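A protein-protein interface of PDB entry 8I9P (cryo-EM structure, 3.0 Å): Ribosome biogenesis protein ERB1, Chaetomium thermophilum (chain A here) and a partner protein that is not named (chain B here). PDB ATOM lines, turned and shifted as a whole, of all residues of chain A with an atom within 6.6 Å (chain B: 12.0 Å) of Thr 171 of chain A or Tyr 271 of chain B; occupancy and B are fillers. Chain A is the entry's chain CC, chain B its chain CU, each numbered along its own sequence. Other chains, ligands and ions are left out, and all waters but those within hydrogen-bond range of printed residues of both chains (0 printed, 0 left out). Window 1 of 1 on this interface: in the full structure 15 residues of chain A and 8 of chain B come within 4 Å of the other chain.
The side-chain carboxylate (OD2) of Asp 270 of chain B is in hydrogen-bond range of the side-chain hydroxyl (OH) of Tyr 188 of chain A (3.2 Å).
N of Phe 272 of chain B is in hydrogen-bond range of OH of Tyr 180 of chain A (2.4 Å).
OE2 of Glu 274 of chain B sits at hydrogen-bond distance from N of Gly 173 of chain A, 2.7 Å away.
O of Tyr 271 of chain B is in hydrogen-bond range of NH1 of Arg 267 of chain B.
A ring nitrogen (ND1) of His 185 of chain A is in hydrogen-bond range of the backbone NH of Gly 187 of chain A (3.1 Å).
Among the printed residues, merely in contact across the chains: Thr 171 of chain A with Tyr 271 of chain B, Ile 172 of chain A with Glu 274 of chain B, Tyr 180 of chain A with Asp 270 of chain B, Tyr 180 of chain A with Tyr 271 of chain B, His 185 of chain A with Asp 270 of chain B, Tyr 188 of chain A with Pro 268 of chain B and Tyr 188 of chain A with Tyr 271 of chain B.
No residue of chain B comes within 4 Å of Pro 168 of chain A.
No residue of chain B comes within 4 Å of Val 169 of chain A.
Of the printed residues of chain B, Thr 171 of chain A touches Tyr 271.
Gly 173 of chain A touches just one residue of chain B: Glu 274.
Printed residues of chain B within 4 Å of Tyr 180 of chain A: Asp 270 (3.2 Å), Tyr 271 (3.2 Å) and Phe 272 (2.4 Å).
Printed residues of chain B within 4 Å of His 185 of chain A: Asp 270 (3.9 Å).
No residue of chain B comes within 4 Å of Gly 187 of chain A.
No residue of chain B comes within 4 Å of Asp 189 of chain A.
No residue of chain B comes within 4 Å of Ile 190 of chain A.
Thr 266 of chain B touches none of the printed residues of chain A.
Arg 267 of chain B touches none of the printed residues of chain A.
Of the printed residues of chain A, Asp 270 of chain B touches Tyr 180 (3.2 Å), His 185 (3.9 Å) and Tyr 188 (3.2 Å).
Of chain A, only Thr 171, Tyr 180 and Tyr 188 come within 4 Å of Tyr 271 of chain B.
Of the printed residues of chain A, Phe 272 of chain B touches Tyr 180 (2.4 Å).
The nearest residue of chain A that does not touch Tyr 271 of chain B is Gly 187 of chain A (5.0 Å).
Of the 12 printed residues of chain A, 6 touch a printed residue of chain B.
Hydrophobic or aromatic side chains of chain A within 4 Å of the printed part of chain B: Ile 172, Tyr 180, His 185 and Tyr 188.
Of the 14 printed residues of chain B, 5 touch a printed residue of chain A.
Printed residues of chain B that touch a printed residue of chain A: Pro 268, Asp 270, Tyr 271, Phe 272 and Glu 274.
Hydrophobic or aromatic side chains of chain B that line the printed part of chain A: Pro 268, Tyr 271 and Phe 272.
Among the printed residues, no Asp or Glu carboxylate lies within 4 Å of a Lys or Arg side-chain nitrogen of the other chain.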
ATOM      1  N   PRO A 168       7.132  12.981  -6.569  1.00  0.00           N
ATOM      2  CA  PRO A 168       8.231  13.861  -6.149  1.00  0.00           C
ATOM      3  C   PRO A 168       8.450  13.838  -4.643  1.00  0.00           C
ATOM      4  O   PRO A 168       7.621  13.374  -3.858  1.00  0.00           O
ATOM      5  CB  PRO A 168       7.776  15.245  -6.624  1.00  0.00           C
ATOM      6  CG  PRO A 168       6.290  15.145  -6.682  1.00  0.00           C
ATOM      7  CD  PRO A 168       6.004  13.744  -7.131  1.00  0.00           C
ATOM      8  N   VAL A 169       9.604  14.372  -4.243  1.00  0.00           N
ATOM      9  CA  VAL A 169      10.057  14.370  -2.859  1.00  0.00           C
ATOM     10  C   VAL A 169       9.983  15.770  -2.241  1.00  0.00           C
ATOM     11  O   VAL A 169      10.665  16.054  -1.263  1.00  0.00           O
ATOM     12  CB  VAL A 169      11.480  13.786  -2.748  1.00  0.00           C
ATOM     13  CG1 VAL A 169      12.002  13.896  -1.322  1.00  0.00           C
ATOM     14  CG2 VAL A 169      11.507  12.333  -3.220  1.00  0.00           C
ATOM     15  N   ASN A 170       9.150  16.647  -2.802  1.00  0.00           N
ATOM     16  CA  ASN A 170       8.982  18.010  -2.315  1.00  0.00           C
ATOM     17  C   ASN A 170       7.623  18.203  -1.632  1.00  0.00           C
ATOM     18  O   ASN A 170       7.394  19.242  -0.999  1.00  0.00           O
ATOM     19  CB  ASN A 170       9.202  18.981  -3.501  1.00  0.00           C
ATOM     20  CG  ASN A 170       8.814  20.413  -3.202  1.00  0.00           C
ATOM     21  OD1 ASN A 170       8.019  21.023  -3.918  1.00  0.00           O
ATOM     22  ND2 ASN A 170       9.363  20.952  -2.121  1.00  0.00           N
ATOM     23  N   THR A 171       6.773  17.164  -1.670  1.00  0.00           N
ATOM     24  CA  THR A 171       5.424  17.060  -1.063  1.00  0.00           C
ATOM     25  C   THR A 171       4.540  18.301  -1.249  1.00  0.00           C
ATOM     26  O   THR A 171       3.897  18.779  -0.314  1.00  0.00           O
ATOM     27  CB  THR A 171       5.479  16.619   0.425  1.00  0.00           C
ATOM     28  OG1 THR A 171       4.149  16.441   0.931  1.00  0.00           O
ATOM     29  CG2 THR A 171       6.253  17.561   1.383  1.00  0.00           C
ATOM     30  N   ILE A 172       4.445  18.799  -2.483  1.00  0.00           N
ATOM     31  CA  ILE A 172       3.371  19.734  -2.814  1.00  0.00           C
ATOM     32  C   ILE A 172       2.662  19.265  -4.081  1.00  0.00           C
ATOM     33  O   ILE A 172       3.075  18.291  -4.721  1.00  0.00           O
ATOM     34  CB  ILE A 172       3.866  21.188  -2.971  1.00  0.00           C
ATOM     35  CG1 ILE A 172       4.758  21.319  -4.199  1.00  0.00           C
ATOM     36  CG2 ILE A 172       4.538  21.728  -1.677  1.00  0.00           C
ATOM     37  CD1 ILE A 172       4.763  22.702  -4.775  1.00  0.00           C
ATOM     38  N   GLY A 173       1.605  19.982  -4.451  1.00  0.00           N
ATOM     39  CA  GLY A 173       0.741  19.681  -5.571  1.00  0.00           C
ATOM     40  C   GLY A 173       0.849  20.802  -6.582  1.00  0.00           C
ATOM     41  O   GLY A 173       1.853  20.917  -7.295  1.00  0.00           O
ATOM     42  N   TYR A 180       6.983  30.496  -1.568  1.00  0.00           N
ATOM     43  CA  TYR A 180       8.350  30.108  -1.211  1.00  0.00           C
ATOM     44  C   TYR A 180       9.434  30.813  -2.018  1.00  0.00           C
ATOM     45  O   TYR A 180      10.576  30.338  -2.027  1.00  0.00           O
ATOM     46  CB  TYR A 180       8.599  28.596  -1.327  1.00  0.00           C
ATOM     47  CG  TYR A 180       7.846  27.719  -0.357  1.00  0.00           C
ATOM     48  CD1 TYR A 180       7.779  28.034   0.991  1.00  0.00           C
ATOM     49  CD2 TYR A 180       7.244  26.543  -0.788  1.00  0.00           C
ATOM     50  CE1 TYR A 180       7.102  27.221   1.878  1.00  0.00           C
ATOM     51  CE2 TYR A 180       6.569  25.722   0.093  1.00  0.00           C
ATOM     52  CZ  TYR A 180       6.503  26.066   1.424  1.00  0.00           C
ATOM     53  OH  TYR A 180       5.835  25.251   2.306  1.00  0.00           O
ATOM     54  N   HIS A 185      13.795  28.054   0.948  1.00  0.00           N
ATOM     55  CA  HIS A 185      13.423  26.677   0.663  1.00  0.00           C
ATOM     56  C   HIS A 185      12.229  26.605  -0.284  1.00  0.00           C
ATOM     57  O   HIS A 185      11.676  27.623  -0.709  1.00  0.00           O
ATOM     58  CB  HIS A 185      13.121  25.940   1.967  1.00  0.00           C
ATOM     59  CG  HIS A 185      11.802  26.298   2.576  1.00  0.00           C
ATOM     60  ND1 HIS A 185      10.828  25.363   2.849  1.00  0.00           N
ATOM     61  CD2 HIS A 185      11.304  27.490   2.986  1.00  0.00           C
ATOM     62  CE1 HIS A 185       9.787  25.961   3.402  1.00  0.00           C
ATOM     63  NE2 HIS A 185      10.048  27.253   3.492  1.00  0.00           N
ATOM     64  N   GLY A 187       9.845  23.895   0.360  1.00  0.00           N
ATOM     65  CA  GLY A 187       8.951  22.985   1.048  1.00  0.00           C
ATOM     66  C   GLY A 187       9.691  22.024   1.963  1.00  0.00           C
ATOM     67  O   GLY A 187      10.915  22.032   2.073  1.00  0.00           O
ATOM     68  N   TYR A 188       8.896  21.200   2.644  1.00  0.00           N
ATOM     69  CA  TYR A 188       9.397  20.169   3.543  1.00  0.00           C
ATOM     70  C   TYR A 188       9.485  18.832   2.801  1.00  0.00           C
ATOM     71  O   TYR A 188       9.376  18.777   1.573  1.00  0.00           O
ATOM     72  CB  TYR A 188       8.507  20.080   4.787  1.00  0.00           C
ATOM     73  CG  TYR A 188       8.809  21.107   5.854  1.00  0.00           C
ATOM     74  CD1 TYR A 188       9.813  20.892   6.790  1.00  0.00           C
ATOM     75  CD2 TYR A 188       8.087  22.291   5.930  1.00  0.00           C
ATOM     76  CE1 TYR A 188      10.090  21.828   7.770  1.00  0.00           C
ATOM     77  CE2 TYR A 188       8.357  23.232   6.904  1.00  0.00           C
ATOM     78  CZ  TYR A 188       9.358  22.996   7.822  1.00  0.00           C
ATOM     79  OH  TYR A 188       9.627  23.933   8.792  1.00  0.00           O
ATOM     80  N   ASP A 189       9.691  17.744   3.541  1.00  0.00           N
ATOM     81  CA  ASP A 189       9.688  16.389   3.001  1.00  0.00           C
ATOM     82  C   ASP A 189       8.870  15.512   3.949  1.00  0.00           C
ATOM     83  O   ASP A 189       8.160  16.017   4.822  1.00  0.00           O
ATOM     84  CB  ASP A 189      11.122  15.882   2.786  1.00  0.00           C
ATOM     85  CG  ASP A 189      11.791  15.425   4.071  1.00  0.00           C
ATOM     86  OD1 ASP A 189      11.613  14.249   4.460  1.00  0.00           O
ATOM     87  OD2 ASP A 189      12.495  16.244   4.692  1.00  0.00           O
ATOM     88  N   ILE A 190       8.965  14.190   3.762  1.00  0.00           N
ATOM     89  CA  ILE A 190       8.154  13.247   4.534  1.00  0.00           C
ATOM     90  C   ILE A 190       8.524  13.293   6.013  1.00  0.00           C
ATOM     91  O   ILE A 190       7.652  13.381   6.887  1.00  0.00           O
ATOM     92  CB  ILE A 190       8.301  11.827   3.955  1.00  0.00           C
ATOM     93  CG1 ILE A 190       7.422  11.666   2.718  1.00  0.00           C
ATOM     94  CG2 ILE A 190       7.930  10.766   4.984  1.00  0.00           C
ATOM     95  CD1 ILE A 190       6.007  12.151   2.920  1.00  0.00           C
ATOM     96  N   PRO B 264       7.156  14.905  14.525  1.00  0.00           N
ATOM     97  CA  PRO B 264       6.643  16.282  14.474  1.00  0.00           C
ATOM     98  C   PRO B 264       5.125  16.333  14.377  1.00  0.00           C
ATOM     99  O   PRO B 264       4.499  15.552  13.657  1.00  0.00           O
ATOM    100  CB  PRO B 264       7.301  16.857  13.215  1.00  0.00           C
ATOM    101  CG  PRO B 264       8.519  16.024  13.006  1.00  0.00           C
ATOM    102  CD  PRO B 264       8.154  14.646  13.472  1.00  0.00           C
ATOM    103  N   PHE B 265       4.540  17.273  15.111  1.00  0.00           N
ATOM    104  CA  PHE B 265       3.094  17.447  15.197  1.00  0.00           C
ATOM    105  C   PHE B 265       2.641  18.838  14.793  1.00  0.00           C
ATOM    106  O   PHE B 265       1.620  18.977  14.114  1.00  0.00           O
ATOM    107  CB  PHE B 265       2.620  17.132  16.633  1.00  0.00           C
ATOM    108  CG  PHE B 265       1.139  17.325  16.859  1.00  0.00           C
ATOM    109  CD1 PHE B 265       0.252  16.296  16.590  1.00  0.00           C
ATOM    110  CD2 PHE B 265       0.634  18.527  17.343  1.00  0.00           C
ATOM    111  CE1 PHE B 265      -1.107  16.461  16.794  1.00  0.00           C
ATOM    112  CE2 PHE B 265      -0.722  18.698  17.544  1.00  0.00           C
ATOM    113  CZ  PHE B 265      -1.593  17.663  17.271  1.00  0.00           C
ATOM    114  N   THR B 266       3.370  19.873  15.194  1.00  0.00           N
ATOM    115  CA  THR B 266       2.940  21.247  14.977  1.00  0.00           C
ATOM    116  C   THR B 266       3.229  21.651  13.538  1.00  0.00           C
ATOM    117  O   THR B 266       4.389  21.653  13.113  1.00  0.00           O
ATOM    118  CB  THR B 266       3.663  22.184  15.941  1.00  0.00           C
ATOM    119  OG1 THR B 266       5.055  21.850  15.972  1.00  0.00           O
ATOM    120  CG2 THR B 266       3.101  22.042  17.343  1.00  0.00           C
ATOM    121  N   ARG B 267       2.188  21.991  12.791  1.00  0.00           N
ATOM    122  CA  ARG B 267       2.400  22.560  11.467  1.00  0.00           C
ATOM    123  C   ARG B 267       2.862  24.001  11.634  1.00  0.00           C
ATOM    124  O   ARG B 267       2.142  24.807  12.240  1.00  0.00           O
ATOM    125  CB  ARG B 267       1.128  22.494  10.626  1.00  0.00           C
ATOM    126  CG  ARG B 267       1.079  23.522   9.499  1.00  0.00           C
ATOM    127  CD  ARG B 267       0.238  23.050   8.331  1.00  0.00           C
ATOM    128  NE  ARG B 267      -0.461  24.155   7.685  1.00  0.00           N
ATOM    129  CZ  ARG B 267      -0.141  24.657   6.500  1.00  0.00           C
ATOM    130  NH1 ARG B 267       0.871  24.178   5.796  1.00  0.00           N
ATOM    131  NH2 ARG B 267      -0.854  25.667   6.010  1.00  0.00           N
ATOM    132  N   PRO B 268       4.042  24.366  11.146  1.00  0.00           N
ATOM    133  CA  PRO B 268       4.524  25.737  11.321  1.00  0.00           C
ATOM    134  C   PRO B 268       4.006  26.662  10.230  1.00  0.00           C
ATOM    135  O   PRO B 268       3.506  26.232   9.189  1.00  0.00           O
ATOM    136  CB  PRO B 268       6.051  25.597  11.249  1.00  0.00           C
ATOM    137  CG  PRO B 268       6.329  24.159  10.843  1.00  0.00           C
ATOM    138  CD  PRO B 268       5.031  23.522  10.461  1.00  0.00           C
ATOM    139  N   THR B 269       4.130  27.964  10.501  1.00  0.00           N
ATOM    140  CA  THR B 269       3.646  28.978   9.571  1.00  0.00           C
ATOM    141  C   THR B 269       4.504  29.086   8.317  1.00  0.00           C
ATOM    142  O   THR B 269       4.006  29.547   7.285  1.00  0.00           O
ATOM    143  CB  THR B 269       3.570  30.339  10.259  1.00  0.00           C
ATOM    144  OG1 THR B 269       4.869  30.706  10.742  1.00  0.00           O
ATOM    145  CG2 THR B 269       2.589  30.297  11.421  1.00  0.00           C
ATOM    146  N   ASP B 270       5.775  28.678   8.373  1.00  0.00           N
ATOM    147  CA  ASP B 270       6.600  28.704   7.171  1.00  0.00           C
ATOM    148  C   ASP B 270       6.210  27.634   6.155  1.00  0.00           C
ATOM    149  O   ASP B 270       6.518  27.794   4.971  1.00  0.00           O
ATOM    150  CB  ASP B 270       8.089  28.595   7.536  1.00  0.00           C
ATOM    151  CG  ASP B 270       8.471  27.254   8.169  1.00  0.00           C
ATOM    152  OD1 ASP B 270       7.596  26.404   8.440  1.00  0.00           O
ATOM    153  OD2 ASP B 270       9.677  27.066   8.436  1.00  0.00           O
ATOM    154  N   TYR B 271       5.548  26.562   6.580  1.00  0.00           N
ATOM    155  CA  TYR B 271       5.133  25.499   5.675  1.00  0.00           C
ATOM    156  C   TYR B 271       3.869  25.923   4.938  1.00  0.00           C
ATOM    157  O   TYR B 271       2.798  26.023   5.543  1.00  0.00           O
ATOM    158  CB  TYR B 271       4.886  24.204   6.451  1.00  0.00           C
ATOM    159  CG  TYR B 271       4.555  23.004   5.594  1.00  0.00           C
ATOM    160  CD1 TYR B 271       5.104  22.861   4.326  1.00  0.00           C
ATOM    161  CD2 TYR B 271       3.702  22.010   6.052  1.00  0.00           C
ATOM    162  CE1 TYR B 271       4.816  21.766   3.538  1.00  0.00           C
ATOM    163  CE2 TYR B 271       3.405  20.902   5.267  1.00  0.00           C
ATOM    164  CZ  TYR B 271       3.965  20.790   4.008  1.00  0.00           C
ATOM    165  OH  TYR B 271       3.678  19.700   3.217  1.00  0.00           O
ATOM    166  N   PHE B 272       3.989  26.160   3.632  1.00  0.00           N
ATOM    167  CA  PHE B 272       2.829  26.400   2.782  1.00  0.00           C
ATOM    168  C   PHE B 272       2.612  25.194   1.882  1.00  0.00           C
ATOM    169  O   PHE B 272       3.530  24.756   1.180  1.00  0.00           O
ATOM    170  CB  PHE B 272       2.968  27.669   1.926  1.00  0.00           C
ATOM    171  CG  PHE B 272       3.231  28.929   2.715  1.00  0.00           C
ATOM    172  CD1 PHE B 272       4.517  29.307   3.066  1.00  0.00           C
ATOM    173  CD2 PHE B 272       2.175  29.745   3.085  1.00  0.00           C
ATOM    174  CE1 PHE B 272       4.736  30.466   3.790  1.00  0.00           C
ATOM    175  CE2 PHE B 272       2.384  30.900   3.802  1.00  0.00           C
ATOM    176  CZ  PHE B 272       3.666  31.264   4.156  1.00  0.00           C
ATOM    177  N   ALA B 273       1.386  24.678   1.899  1.00  0.00           N
ATOM    178  CA  ALA B 273       0.972  23.552   1.086  1.00  0.00           C
ATOM    179  C   ALA B 273      -0.357  23.917   0.444  1.00  0.00           C
ATOM    180  O   ALA B 273      -0.891  25.011   0.634  1.00  0.00           O
ATOM    181  CB  ALA B 273       0.892  22.260   1.914  1.00  0.00           C
ATOM    182  N   GLU B 274      -0.887  22.996  -0.342  1.00  0.00           N
ATOM    183  CA  GLU B 274      -2.119  23.244  -1.078  1.00  0.00           C
ATOM    184  C   GLU B 274      -3.295  23.206  -0.103  1.00  0.00           C
ATOM    185  O   GLU B 274      -3.091  23.035   1.103  1.00  0.00           O
ATOM    186  CB  GLU B 274      -2.240  22.211  -2.180  1.00  0.00           C
ATOM    187  CG  GLU B 274      -1.408  22.568  -3.414  1.00  0.00           C
ATOM    188  CD  GLU B 274       0.158  22.568  -3.186  1.00  0.00           C
ATOM    189  OE1 GLU B 274       0.710  22.589  -2.062  1.00  0.00           O
ATOM    190  OE2 GLU B 274       0.862  22.521  -4.194  1.00  0.00           O
ATOM    191  N   MET B 275      -4.521  23.437  -0.580  1.00  0.00           N
ATOM    192  CA  MET B 275      -5.565  23.547   0.429  1.00  0.00           C
ATOM    193  C   MET B 275      -6.564  22.410   0.116  1.00  0.00           C
ATOM    194  O   MET B 275      -6.503  21.803  -0.962  1.00  0.00           O
ATOM    195  CB  MET B 275      -6.229  24.936   0.365  1.00  0.00           C
ATOM    196  CG  MET B 275      -5.314  26.130   0.746  1.00  0.00           C
ATOM    197  SD  MET B 275      -4.820  25.751   2.480  1.00  0.00           S
ATOM    198  CE  MET B 275      -6.285  25.869   3.492  1.00  0.00           C
ATOM    199  N   VAL B 276      -7.422  22.048   1.077  1.00  0.00           N
ATOM    200  CA  VAL B 276      -8.424  21.003   0.810  1.00  0.00           C
ATOM    201  C   VAL B 276      -9.475  21.490  -0.175  1.00  0.00           C
ATOM    202  O   VAL B 276      -9.900  20.746  -1.070  1.00  0.00           O
ATOM    203  CB  VAL B 276      -9.059  20.496   2.123  1.00  0.00           C
ATOM    204  CG1 VAL B 276     -10.549  20.263   2.017  1.00  0.00           C
ATOM    205  CG2 VAL B 276      -8.467  19.158   2.485  1.00  0.00           C
ATOM    206  N   ASP B 279      -8.984  28.284  -2.726  1.00  0.00           N
ATOM    207  CA  ASP B 279      -8.974  29.551  -2.009  1.00  0.00           C
ATOM    208  C   ASP B 279     -10.138  30.449  -2.406  1.00  0.00           C
ATOM    209  O   ASP B 279     -10.428  31.420  -1.698  1.00  0.00           O
ATOM    210  CB  ASP B 279      -7.638  30.252  -2.232  1.00  0.00           C
ATOM    211  CG  ASP B 279      -6.603  29.834  -1.211  1.00  0.00           C
ATOM    212  OD1 ASP B 279      -6.863  28.860  -0.473  1.00  0.00           O
ATOM    213  OD2 ASP B 279      -5.529  30.469  -1.154  1.00  0.00           O
